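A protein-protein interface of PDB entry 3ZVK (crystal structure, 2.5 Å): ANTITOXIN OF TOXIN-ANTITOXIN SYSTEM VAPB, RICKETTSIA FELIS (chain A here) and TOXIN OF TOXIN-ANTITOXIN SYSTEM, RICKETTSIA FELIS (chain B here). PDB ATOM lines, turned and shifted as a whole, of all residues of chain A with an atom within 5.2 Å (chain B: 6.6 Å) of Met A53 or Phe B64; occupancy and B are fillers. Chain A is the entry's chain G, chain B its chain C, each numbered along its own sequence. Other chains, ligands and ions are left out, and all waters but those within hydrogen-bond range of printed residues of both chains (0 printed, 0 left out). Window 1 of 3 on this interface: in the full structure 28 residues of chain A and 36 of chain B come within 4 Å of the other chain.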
ATOM      1  N   TRP A  46       9.612   4.476  22.935  1.00  0.00           N
ATOM      2  CA  TRP A  46       9.076   3.992  21.658  1.00  0.00           C
ATOM      3  C   TRP A  46       9.571   2.586  21.290  1.00  0.00           C
ATOM      4  O   TRP A  46       8.823   1.832  20.669  1.00  0.00           O
ATOM      5  CB  TRP A  46       9.301   5.007  20.529  1.00  0.00           C
ATOM      6  CG  TRP A  46       8.242   6.070  20.461  1.00  0.00           C
ATOM      7  CD1 TRP A  46       8.376   7.387  20.783  1.00  0.00           C
ATOM      8  CD2 TRP A  46       6.867   5.887  20.079  1.00  0.00           C
ATOM      9  NE1 TRP A  46       7.186   8.050  20.569  1.00  0.00           N
ATOM     10  CE2 TRP A  46       6.234   7.145  20.177  1.00  0.00           C
ATOM     11  CE3 TRP A  46       6.118   4.783  19.634  1.00  0.00           C
ATOM     12  CZ2 TRP A  46       4.900   7.341  19.810  1.00  0.00           C
ATOM     13  CZ3 TRP A  46       4.782   4.964  19.332  1.00  0.00           C
ATOM     14  CH2 TRP A  46       4.188   6.237  19.396  1.00  0.00           C
ATOM     15  N   ASP A  48      10.244   0.201  23.580  1.00  0.00           N
ATOM     16  CA  ASP A  48       9.450  -0.645  24.454  1.00  0.00           C
ATOM     17  C   ASP A  48       8.007  -0.753  23.952  1.00  0.00           C
ATOM     18  O   ASP A  48       7.379  -1.786  24.155  1.00  0.00           O
ATOM     19  CB  ASP A  48       9.537  -0.158  25.910  1.00  0.00           C
ATOM     20  CG  ASP A  48      10.950  -0.047  26.484  1.00  0.00           C
ATOM     21  OD1 ASP A  48      11.816  -0.884  26.120  1.00  0.00           O
ATOM     22  OD2 ASP A  48      11.179   0.852  27.333  1.00  0.00           O
ATOM     23  N   VAL A  49       7.497   0.288  23.270  1.00  0.00           N
ATOM     24  CA  VAL A  49       6.161   0.312  22.656  1.00  0.00           C
ATOM     25  C   VAL A  49       6.134  -0.732  21.517  1.00  0.00           C
ATOM     26  O   VAL A  49       5.232  -1.577  21.473  1.00  0.00           O
ATOM     27  CB  VAL A  49       5.784   1.756  22.150  1.00  0.00           C
ATOM     28  CG1 VAL A  49       4.656   1.725  21.127  1.00  0.00           C
ATOM     29  CG2 VAL A  49       5.421   2.675  23.312  1.00  0.00           C
ATOM     30  N   PHE A  50       7.156  -0.678  20.635  1.00  0.00           N
ATOM     31  CA  PHE A  50       7.305  -1.547  19.467  1.00  0.00           C
ATOM     32  C   PHE A  50       7.579  -2.993  19.859  1.00  0.00           C
ATOM     33  O   PHE A  50       7.075  -3.888  19.190  1.00  0.00           O
ATOM     34  CB  PHE A  50       8.358  -0.990  18.502  1.00  0.00           C
ATOM     35  CG  PHE A  50       7.857   0.009  17.483  1.00  0.00           C
ATOM     36  CD1 PHE A  50       7.217   1.183  17.883  1.00  0.00           C
ATOM     37  CD2 PHE A  50       8.057  -0.205  16.126  1.00  0.00           C
ATOM     38  CE1 PHE A  50       6.769   2.113  16.934  1.00  0.00           C
ATOM     39  CE2 PHE A  50       7.603   0.717  15.180  1.00  0.00           C
ATOM     40  CZ  PHE A  50       6.957   1.865  15.585  1.00  0.00           C
ATOM     41  N   GLN A  51       8.328  -3.221  20.959  1.00  0.00           N
ATOM     42  CA  GLN A  51       8.638  -4.543  21.505  1.00  0.00           C
ATOM     43  C   GLN A  51       7.379  -5.211  22.056  1.00  0.00           C
ATOM     44  O   GLN A  51       7.155  -6.387  21.788  1.00  0.00           O
ATOM     45  CB  GLN A  51       9.698  -4.440  22.615  1.00  0.00           C
ATOM     46  CG  GLN A  51      11.135  -4.571  22.117  1.00  0.00           C
ATOM     47  CD  GLN A  51      12.192  -4.193  23.144  1.00  0.00           C
ATOM     48  OE1 GLN A  51      11.947  -4.104  24.361  1.00  0.00           O
ATOM     49  NE2 GLN A  51      13.404  -3.941  22.661  1.00  0.00           N
ATOM     50  N   GLU A  52       6.557  -4.456  22.814  1.00  0.00           N
ATOM     51  CA  GLU A  52       5.296  -4.928  23.410  1.00  0.00           C
ATOM     52  C   GLU A  52       4.246  -5.311  22.356  1.00  0.00           C
ATOM     53  O   GLU A  52       3.542  -6.306  22.543  1.00  0.00           O
ATOM     54  CB  GLU A  52       4.752  -3.918  24.444  1.00  0.00           C
ATOM     55  CG  GLU A  52       5.339  -4.161  25.825  1.00  0.00           C
ATOM     56  CD  GLU A  52       5.152  -3.067  26.854  1.00  0.00           C
ATOM     57  OE1 GLU A  52       4.124  -3.093  27.568  1.00  0.00           O
ATOM     58  OE2 GLU A  52       6.077  -2.238  27.010  1.00  0.00           O
ATOM     59  N   MET A  53       4.183  -4.552  21.231  1.00  0.00           N
ATOM     60  CA  MET A  53       3.290  -4.830  20.093  1.00  0.00           C
ATOM     61  C   MET A  53       3.748  -6.108  19.362  1.00  0.00           C
ATOM     62  O   MET A  53       2.910  -6.882  18.901  1.00  0.00           O
ATOM     63  CB  MET A  53       3.284  -3.670  19.084  1.00  0.00           C
ATOM     64  CG  MET A  53       2.617  -2.402  19.575  1.00  0.00           C
ATOM     65  SD  MET A  53       2.285  -1.251  18.226  1.00  0.00           S
ATOM     66  CE  MET A  53       3.898  -0.792  17.739  1.00  0.00           C
ATOM     67  N   ALA A  54       5.076  -6.310  19.239  1.00  0.00           N
ATOM     68  CA  ALA A  54       5.684  -7.468  18.579  1.00  0.00           C
ATOM     69  C   ALA A  54       5.406  -8.785  19.339  1.00  0.00           C
ATOM     70  O   ALA A  54       5.357  -9.845  18.711  1.00  0.00           O
ATOM     71  CB  ALA A  54       7.180  -7.253  18.435  1.00  0.00           C
ATOM     72  N   GLU A  55       5.198  -8.705  20.677  1.00  0.00           N
ATOM     73  CA  GLU A  55       4.880  -9.847  21.545  1.00  0.00           C
ATOM     74  C   GLU A  55       3.464 -10.359  21.271  1.00  0.00           C
ATOM     75  O   GLU A  55       3.223 -11.561  21.311  1.00  0.00           O
ATOM     76  CB  GLU A  55       5.043  -9.475  23.030  1.00  0.00           C
ATOM     77  CG  GLU A  55       6.492  -9.329  23.470  1.00  0.00           C
ATOM     78  CD  GLU A  55       6.707  -8.897  24.908  1.00  0.00           C
ATOM     79  OE1 GLU A  55       5.986  -7.986  25.379  1.00  0.00           O
ATOM     80  OE2 GLU A  55       7.621  -9.455  25.558  1.00  0.00           O
ATOM     81  N   ILE A  56       2.535  -9.444  20.969  1.00  0.00           N
ATOM     82  CA  ILE A  56       1.137  -9.760  20.657  1.00  0.00           C
ATOM     83  C   ILE A  56       1.015 -10.370  19.229  1.00  0.00           C
ATOM     84  O   ILE A  56       1.387  -9.734  18.231  1.00  0.00           O
ATOM     85  CB  ILE A  56       0.217  -8.516  20.866  1.00  0.00           C
ATOM     86  CG1 ILE A  56       0.216  -8.046  22.333  1.00  0.00           C
ATOM     87  CG2 ILE A  56      -1.204  -8.783  20.371  1.00  0.00           C
ATOM     88  CD1 ILE A  56       0.073  -6.584  22.497  1.00  0.00           C
ATOM     89  N   LEU B   5       1.221  11.822  12.546  1.00  0.00           N
ATOM     90  CA  LEU B   5       1.338  10.569  11.798  1.00  0.00           C
ATOM     91  C   LEU B   5       0.079  10.261  10.970  1.00  0.00           C
ATOM     92  O   LEU B   5      -1.050  10.350  11.495  1.00  0.00           O
ATOM     93  CB  LEU B   5       1.668   9.360  12.717  1.00  0.00           C
ATOM     94  CG  LEU B   5       2.761   9.546  13.793  1.00  0.00           C
ATOM     95  CD1 LEU B   5       2.869   8.312  14.686  1.00  0.00           C
ATOM     96  CD2 LEU B   5       4.106   9.871  13.178  1.00  0.00           C
ATOM     97  N   ILE B   9       1.436   5.149   7.966  1.00  0.00           N
ATOM     98  CA  ILE B   9       2.570   5.066   8.899  1.00  0.00           C
ATOM     99  C   ILE B   9       2.128   4.248  10.112  1.00  0.00           C
ATOM    100  O   ILE B   9       2.862   3.355  10.541  1.00  0.00           O
ATOM    101  CB  ILE B   9       3.113   6.486   9.295  1.00  0.00           C
ATOM    102  CG1 ILE B   9       4.050   7.056   8.229  1.00  0.00           C
ATOM    103  CG2 ILE B   9       3.782   6.534  10.678  1.00  0.00           C
ATOM    104  CD1 ILE B   9       5.510   6.369   8.058  1.00  0.00           C
ATOM    105  N   CYS B  10       0.899   4.505  10.601  1.00  0.00           N
ATOM    106  CA  CYS B  10       0.329   3.829  11.769  1.00  0.00           C
ATOM    107  C   CYS B  10       0.063   2.377  11.551  1.00  0.00           C
ATOM    108  O   CYS B  10       0.523   1.566  12.341  1.00  0.00           O
ATOM    109  CB  CYS B  10      -0.895   4.564  12.305  1.00  0.00           C
ATOM    110  SG  CYS B  10      -0.523   6.217  12.932  1.00  0.00           S
ATOM    111  N   VAL B  11      -0.629   2.039  10.463  1.00  0.00           N
ATOM    112  CA  VAL B  11      -0.940   0.667  10.068  1.00  0.00           C
ATOM    113  C   VAL B  11       0.362  -0.155   9.944  1.00  0.00           C
ATOM    114  O   VAL B  11       0.427  -1.248  10.506  1.00  0.00           O
ATOM    115  CB  VAL B  11      -1.791   0.637   8.769  1.00  0.00           C
ATOM    116  CG1 VAL B  11      -1.906  -0.783   8.187  1.00  0.00           C
ATOM    117  CG2 VAL B  11      -3.172   1.235   9.004  1.00  0.00           C
ATOM    118  N   ALA B  13       3.302   0.552  11.348  1.00  0.00           N
ATOM    119  CA  ALA B  13       3.903   0.508  12.685  1.00  0.00           C
ATOM    120  C   ALA B  13       3.286  -0.619  13.525  1.00  0.00           C
ATOM    121  O   ALA B  13       4.029  -1.397  14.124  1.00  0.00           O
ATOM    122  CB  ALA B  13       3.729   1.840  13.388  1.00  0.00           C
ATOM    123  N   ILE B  14       1.941  -0.729  13.539  1.00  0.00           N
ATOM    124  CA  ILE B  14       1.225  -1.767  14.288  1.00  0.00           C
ATOM    125  C   ILE B  14       1.443  -3.157  13.684  1.00  0.00           C
ATOM    126  O   ILE B  14       1.798  -4.083  14.411  1.00  0.00           O
ATOM    127  CB  ILE B  14      -0.277  -1.411  14.500  1.00  0.00           C
ATOM    128  CG1 ILE B  14      -0.413  -0.095  15.320  1.00  0.00           C
ATOM    129  CG2 ILE B  14      -1.049  -2.576  15.174  1.00  0.00           C
ATOM    130  CD1 ILE B  14      -1.717   0.593  15.201  1.00  0.00           C
ATOM    131  N   ASN B  15       1.284  -3.300  12.364  1.00  0.00           N
ATOM    132  CA  ASN B  15       1.474  -4.585  11.705  1.00  0.00           C
ATOM    133  C   ASN B  15       2.908  -5.062  11.634  1.00  0.00           C
ATOM    134  O   ASN B  15       3.167  -6.201  12.003  1.00  0.00           O
ATOM    135  CB  ASN B  15       0.844  -4.594  10.315  1.00  0.00           C
ATOM    136  CG  ASN B  15      -0.665  -4.563  10.298  1.00  0.00           C
ATOM    137  OD1 ASN B  15      -1.349  -4.959  11.238  1.00  0.00           O
ATOM    138  ND2 ASN B  15      -1.220  -4.135   9.189  1.00  0.00           N
ATOM    139  N   HIS B  17       5.877  -3.244  12.855  1.00  0.00           N
ATOM    140  CA  HIS B  17       6.751  -2.685  13.906  1.00  0.00           C
ATOM    141  C   HIS B  17       8.248  -2.591  13.485  1.00  0.00           C
ATOM    142  O   HIS B  17       9.093  -3.286  14.056  1.00  0.00           O
ATOM    143  CB  HIS B  17       6.540  -3.377  15.271  1.00  0.00           C
ATOM    144  CG  HIS B  17       6.380  -4.863  15.192  1.00  0.00           C
ATOM    145  ND1 HIS B  17       7.447  -5.700  14.926  1.00  0.00           N
ATOM    146  CD2 HIS B  17       5.266  -5.608  15.351  1.00  0.00           C
ATOM    147  CE1 HIS B  17       6.941  -6.921  14.905  1.00  0.00           C
ATOM    148  NE2 HIS B  17       5.637  -6.913  15.168  1.00  0.00           N
ATOM    149  N   LEU B  25      10.875   7.961  15.754  1.00  0.00           N
ATOM    150  CA  LEU B  25       9.909   8.420  16.755  1.00  0.00           C
ATOM    151  C   LEU B  25      10.610   8.861  18.029  1.00  0.00           C
ATOM    152  O   LEU B  25      10.385   9.980  18.481  1.00  0.00           O
ATOM    153  CB  LEU B  25       8.810   7.364  17.041  1.00  0.00           C
ATOM    154  CG  LEU B  25       7.759   7.148  15.961  1.00  0.00           C
ATOM    155  CD1 LEU B  25       7.069   5.853  16.156  1.00  0.00           C
ATOM    156  CD2 LEU B  25       6.745   8.246  15.943  1.00  0.00           C
ATOM    157  N   ILE B  36      -1.524  12.125  16.453  1.00  0.00           N
ATOM    158  CA  ILE B  36      -2.419  11.607  15.421  1.00  0.00           C
ATOM    159  C   ILE B  36      -3.730  12.363  15.512  1.00  0.00           C
ATOM    160  O   ILE B  36      -4.174  12.755  16.590  1.00  0.00           O
ATOM    161  CB  ILE B  36      -2.664  10.054  15.363  1.00  0.00           C
ATOM    162  CG1 ILE B  36      -3.403   9.496  16.618  1.00  0.00           C
ATOM    163  CG2 ILE B  36      -1.414   9.283  15.013  1.00  0.00           C
ATOM    164  CD1 ILE B  36      -4.128   8.166  16.403  1.00  0.00           C
ATOM    165  N   LEU B  44      -8.054   3.494  12.397  1.00  0.00           N
ATOM    166  CA  LEU B  44      -7.396   2.412  13.137  1.00  0.00           C
ATOM    167  C   LEU B  44      -8.378   1.613  13.978  1.00  0.00           C
ATOM    168  O   LEU B  44      -8.222   0.397  14.080  1.00  0.00           O
ATOM    169  CB  LEU B  44      -6.235   2.916  13.997  1.00  0.00           C
ATOM    170  CG  LEU B  44      -5.111   3.648  13.302  1.00  0.00           C
ATOM    171  CD1 LEU B  44      -4.116   4.184  14.331  1.00  0.00           C
ATOM    172  CD2 LEU B  44      -4.425   2.772  12.261  1.00  0.00           C
ATOM    173  N   SER B  59      -5.405  -4.236  21.777  1.00  0.00           N
ATOM    174  CA  SER B  59      -4.259  -4.203  22.687  1.00  0.00           C
ATOM    175  C   SER B  59      -3.057  -3.543  22.037  1.00  0.00           C
ATOM    176  O   SER B  59      -2.474  -2.649  22.651  1.00  0.00           O
ATOM    177  CB  SER B  59      -3.899  -5.604  23.159  1.00  0.00           C
ATOM    178  OG  SER B  59      -4.938  -6.125  23.971  1.00  0.00           O
ATOM    179  N   LYS B  60      -2.717  -3.944  20.781  1.00  0.00           N
ATOM    180  CA  LYS B  60      -1.607  -3.386  19.989  1.00  0.00           C
ATOM    181  C   LYS B  60      -1.829  -1.901  19.716  1.00  0.00           C
ATOM    182  O   LYS B  60      -0.904  -1.108  19.892  1.00  0.00           O
ATOM    183  CB  LYS B  60      -1.454  -4.133  18.668  1.00  0.00           C
ATOM    184  CG  LYS B  60      -0.715  -5.443  18.800  1.00  0.00           C
ATOM    185  CD  LYS B  60      -0.785  -6.254  17.518  1.00  0.00           C
ATOM    186  CE  LYS B  60       0.318  -5.901  16.562  1.00  0.00           C
ATOM    187  NZ  LYS B  60       0.074  -6.497  15.222  1.00  0.00           N
ATOM    188  N   LEU B  61      -3.063  -1.528  19.313  1.00  0.00           N
ATOM    189  CA  LEU B  61      -3.430  -0.136  19.079  1.00  0.00           C
ATOM    190  C   LEU B  61      -3.291   0.685  20.388  1.00  0.00           C
ATOM    191  O   LEU B  61      -2.700   1.766  20.348  1.00  0.00           O
ATOM    192  CB  LEU B  61      -4.858  -0.047  18.494  1.00  0.00           C
ATOM    193  CG  LEU B  61      -5.470   1.356  18.278  1.00  0.00           C
ATOM    194  CD1 LEU B  61      -4.594   2.224  17.404  1.00  0.00           C
ATOM    195  CD2 LEU B  61      -6.832   1.262  17.679  1.00  0.00           C
ATOM    196  N   ASP B  62      -3.779   0.145  21.544  1.00  0.00           N
ATOM    197  CA  ASP B  62      -3.702   0.803  22.853  1.00  0.00           C
ATOM    198  C   ASP B  62      -2.255   1.104  23.253  1.00  0.00           C
ATOM    199  O   ASP B  62      -1.976   2.213  23.705  1.00  0.00           O
ATOM    200  CB  ASP B  62      -4.410  -0.035  23.935  1.00  0.00           C
ATOM    201  CG  ASP B  62      -5.918  -0.186  23.791  1.00  0.00           C
ATOM    202  OD1 ASP B  62      -6.516   0.512  22.934  1.00  0.00           O
ATOM    203  OD2 ASP B  62      -6.498  -1.016  24.517  1.00  0.00           O
ATOM    204  N   ILE B  63      -1.333   0.140  23.024  1.00  0.00           N
ATOM    205  CA  ILE B  63       0.107   0.257  23.282  1.00  0.00           C
ATOM    206  C   ILE B  63       0.732   1.347  22.380  1.00  0.00           C
ATOM    207  O   ILE B  63       1.545   2.150  22.838  1.00  0.00           O
ATOM    208  CB  ILE B  63       0.787  -1.136  23.109  1.00  0.00           C
ATOM    209  CG1 ILE B  63       0.433  -2.053  24.288  1.00  0.00           C
ATOM    210  CG2 ILE B  63       2.306  -1.020  22.965  1.00  0.00           C
ATOM    211  CD1 ILE B  63       0.575  -3.476  24.036  1.00  0.00           C
ATOM    212  N   PHE B  64       0.337   1.363  21.108  1.00  0.00           N
ATOM    213  CA  PHE B  64       0.812   2.317  20.115  1.00  0.00           C
ATOM    214  C   PHE B  64       0.437   3.752  20.503  1.00  0.00           C
ATOM    215  O   PHE B  64       1.284   4.646  20.400  1.00  0.00           O
ATOM    216  CB  PHE B  64       0.288   1.943  18.712  1.00  0.00           C
ATOM    217  CG  PHE B  64       0.830   2.835  17.624  1.00  0.00           C
ATOM    218  CD1 PHE B  64       2.163   2.747  17.229  1.00  0.00           C
ATOM    219  CD2 PHE B  64       0.020   3.799  17.021  1.00  0.00           C
ATOM    220  CE1 PHE B  64       2.680   3.607  16.260  1.00  0.00           C
ATOM    221  CE2 PHE B  64       0.530   4.646  16.034  1.00  0.00           C
ATOM    222  CZ  PHE B  64       1.854   4.535  15.649  1.00  0.00           C
ATOM    223  N   LEU B  65      -0.806   3.947  21.009  1.00  0.00           N
ATOM    224  CA  LEU B  65      -1.345   5.239  21.443  1.00  0.00           C
ATOM    225  C   LEU B  65      -0.764   5.766  22.748  1.00  0.00           C
ATOM    226  O   LEU B  65      -0.878   6.969  23.000  1.00  0.00           O
ATOM    227  CB  LEU B  65      -2.889   5.202  21.559  1.00  0.00           C
ATOM    228  CG  LEU B  65      -3.705   4.783  20.317  1.00  0.00           C
ATOM    229  CD1 LEU B  65      -5.151   4.570  20.672  1.00  0.00           C
ATOM    230  CD2 LEU B  65      -3.556   5.787  19.169  1.00  0.00           C
ATOM    231  N   SER B  66      -0.154   4.886  23.580  1.00  0.00           N
ATOM    232  CA  SER B  66       0.366   5.257  24.896  1.00  0.00           C
ATOM    233  C   SER B  66       1.358   6.399  24.884  1.00  0.00           C
ATOM    234  O   SER B  66       1.442   7.095  25.899  1.00  0.00           O
ATOM    235  CB  SER B  66       0.940   4.047  25.631  1.00  0.00           C
ATOM    236  OG  SER B  66       2.096   3.544  24.987  1.00  0.00           O
ATOM    237  N   ARG B  67       2.131   6.587  23.771  1.00  0.00           N
ATOM    238  CA  ARG B  67       3.165   7.632  23.737  1.00  0.00           C
ATOM    239  C   ARG B  67       2.921   8.752  22.733  1.00  0.00           C
ATOM    240  O   ARG B  67       3.813   9.572  22.471  1.00  0.00           O
ATOM    241  CB  ARG B  67       4.583   7.041  23.658  1.00  0.00           C
ATOM    242  CG  ARG B  67       4.960   6.204  24.888  1.00  0.00           C
ATOM    243  CD  ARG B  67       6.440   5.862  24.904  1.00  0.00           C
ATOM    244  NE  ARG B  67       7.268   7.020  25.254  1.00  0.00           N
ATOM    245  CZ  ARG B  67       7.477   7.456  26.495  1.00  0.00           C
ATOM    246  NH1 ARG B  67       6.921   6.830  27.531  1.00  0.00           N
ATOM    247  NH2 ARG B  67       8.238   8.522  26.711  1.00  0.00           N
ATOM    248  N   LEU B  68       1.690   8.821  22.211  1.00  0.00           N
ATOM    249  CA  LEU B  68       1.327   9.889  21.294  1.00  0.00           C
ATOM    250  C   LEU B  68       0.120  10.703  21.795  1.00  0.00           C
ATOM    251  O   LEU B  68      -0.523  10.306  22.763  1.00  0.00           O
ATOM    252  CB  LEU B  68       1.307   9.425  19.804  1.00  0.00           C
ATOM    253  CG  LEU B  68       0.065   8.868  19.074  1.00  0.00           C
ATOM    254  CD1 LEU B  68       0.446   7.790  18.109  1.00  0.00           C
ATOM    255  CD2 LEU B  68      -1.032   8.424  19.989  1.00  0.00           C
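Of the 21 printed residues of chain B, 8 touch a printed residue of chain A. Printed residues of chain B that touch a printed residue of chain A: Ala B13, His B17, Leu B25, Lys B60, Ile B63, Phe B64, Ser B66 and Arg B67. Hydrophobic or aromatic side chains of chain B that line the printed part of chain A: Ala B13, His B17, Leu B25, Ile B63 and Phe B64. Of the 10 printed residues of chain A, 6 touch a printed residue of chain B. Printed residues of chain A that touch a printed residue of chain B: Trp A46, Val A49, Phe A50, Met A53, Ala A54 and Ile A56.
Printed residues of chain B within 4 Å of Phe A50: Ala B13, His B17 and Leu B25. Met A53 touches just these residues of chain B: Ala B13, Lys B60, Ile B63 and Phe B64. Printed residues of chain B within 4 Å of Ala A54: His B17 (3.5 Å). Val B11 touches none of the printed residues of chain A. Printed residues of chain A within 4 Å of Phe B64: Trp A46 (3.5 Å) and Met A53 (3.8 Å). The nearest residue of chain B that does not touch Met A53 is Ile B14 (4.1 Å). The nearest printed residue of chain A that does not touch Phe B64 is Val A49 (4.02 Å). The nearest printed residue of chain A that does not touch Ala B13 is Trp A46 (6.8 Å).
SD of Met A53 sits close to O of Lys B60 (3.6 Å).
The backbone carbonyl oxygen (O) of Ile B14 is in hydrogen-bond range of the side-chain amino group (NZ) of Lys B60 (3.1 Å). OG of Ser B66 lies within hydrogen-bond range of O of Ile B63, 2.6 Å away.
CB of Leu B25 touches CG of Trp A46, 3.7 Å away. Trp A46 touches Phe B64. O of Val A49 touches CG2 of Ile B63 (3.3 Å). CD of Arg B67 touches CG2 of Val A49 (3.7 Å). CB of Ala B13 touches CZ of Phe A50, 3.9 Å away. CD1 of Leu B25 touches CE1 of Phe A50, 3.8 Å away. CG of Met A53 touches CG2 of Ile B63, 3.7 Å away. Met A53 touches Phe B64 (SD to CB, 3.8 Å). Ile A56 touches Lys B60. Ile B63 touches Ile A56 (CD1 to CD1, 3.5 Å).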
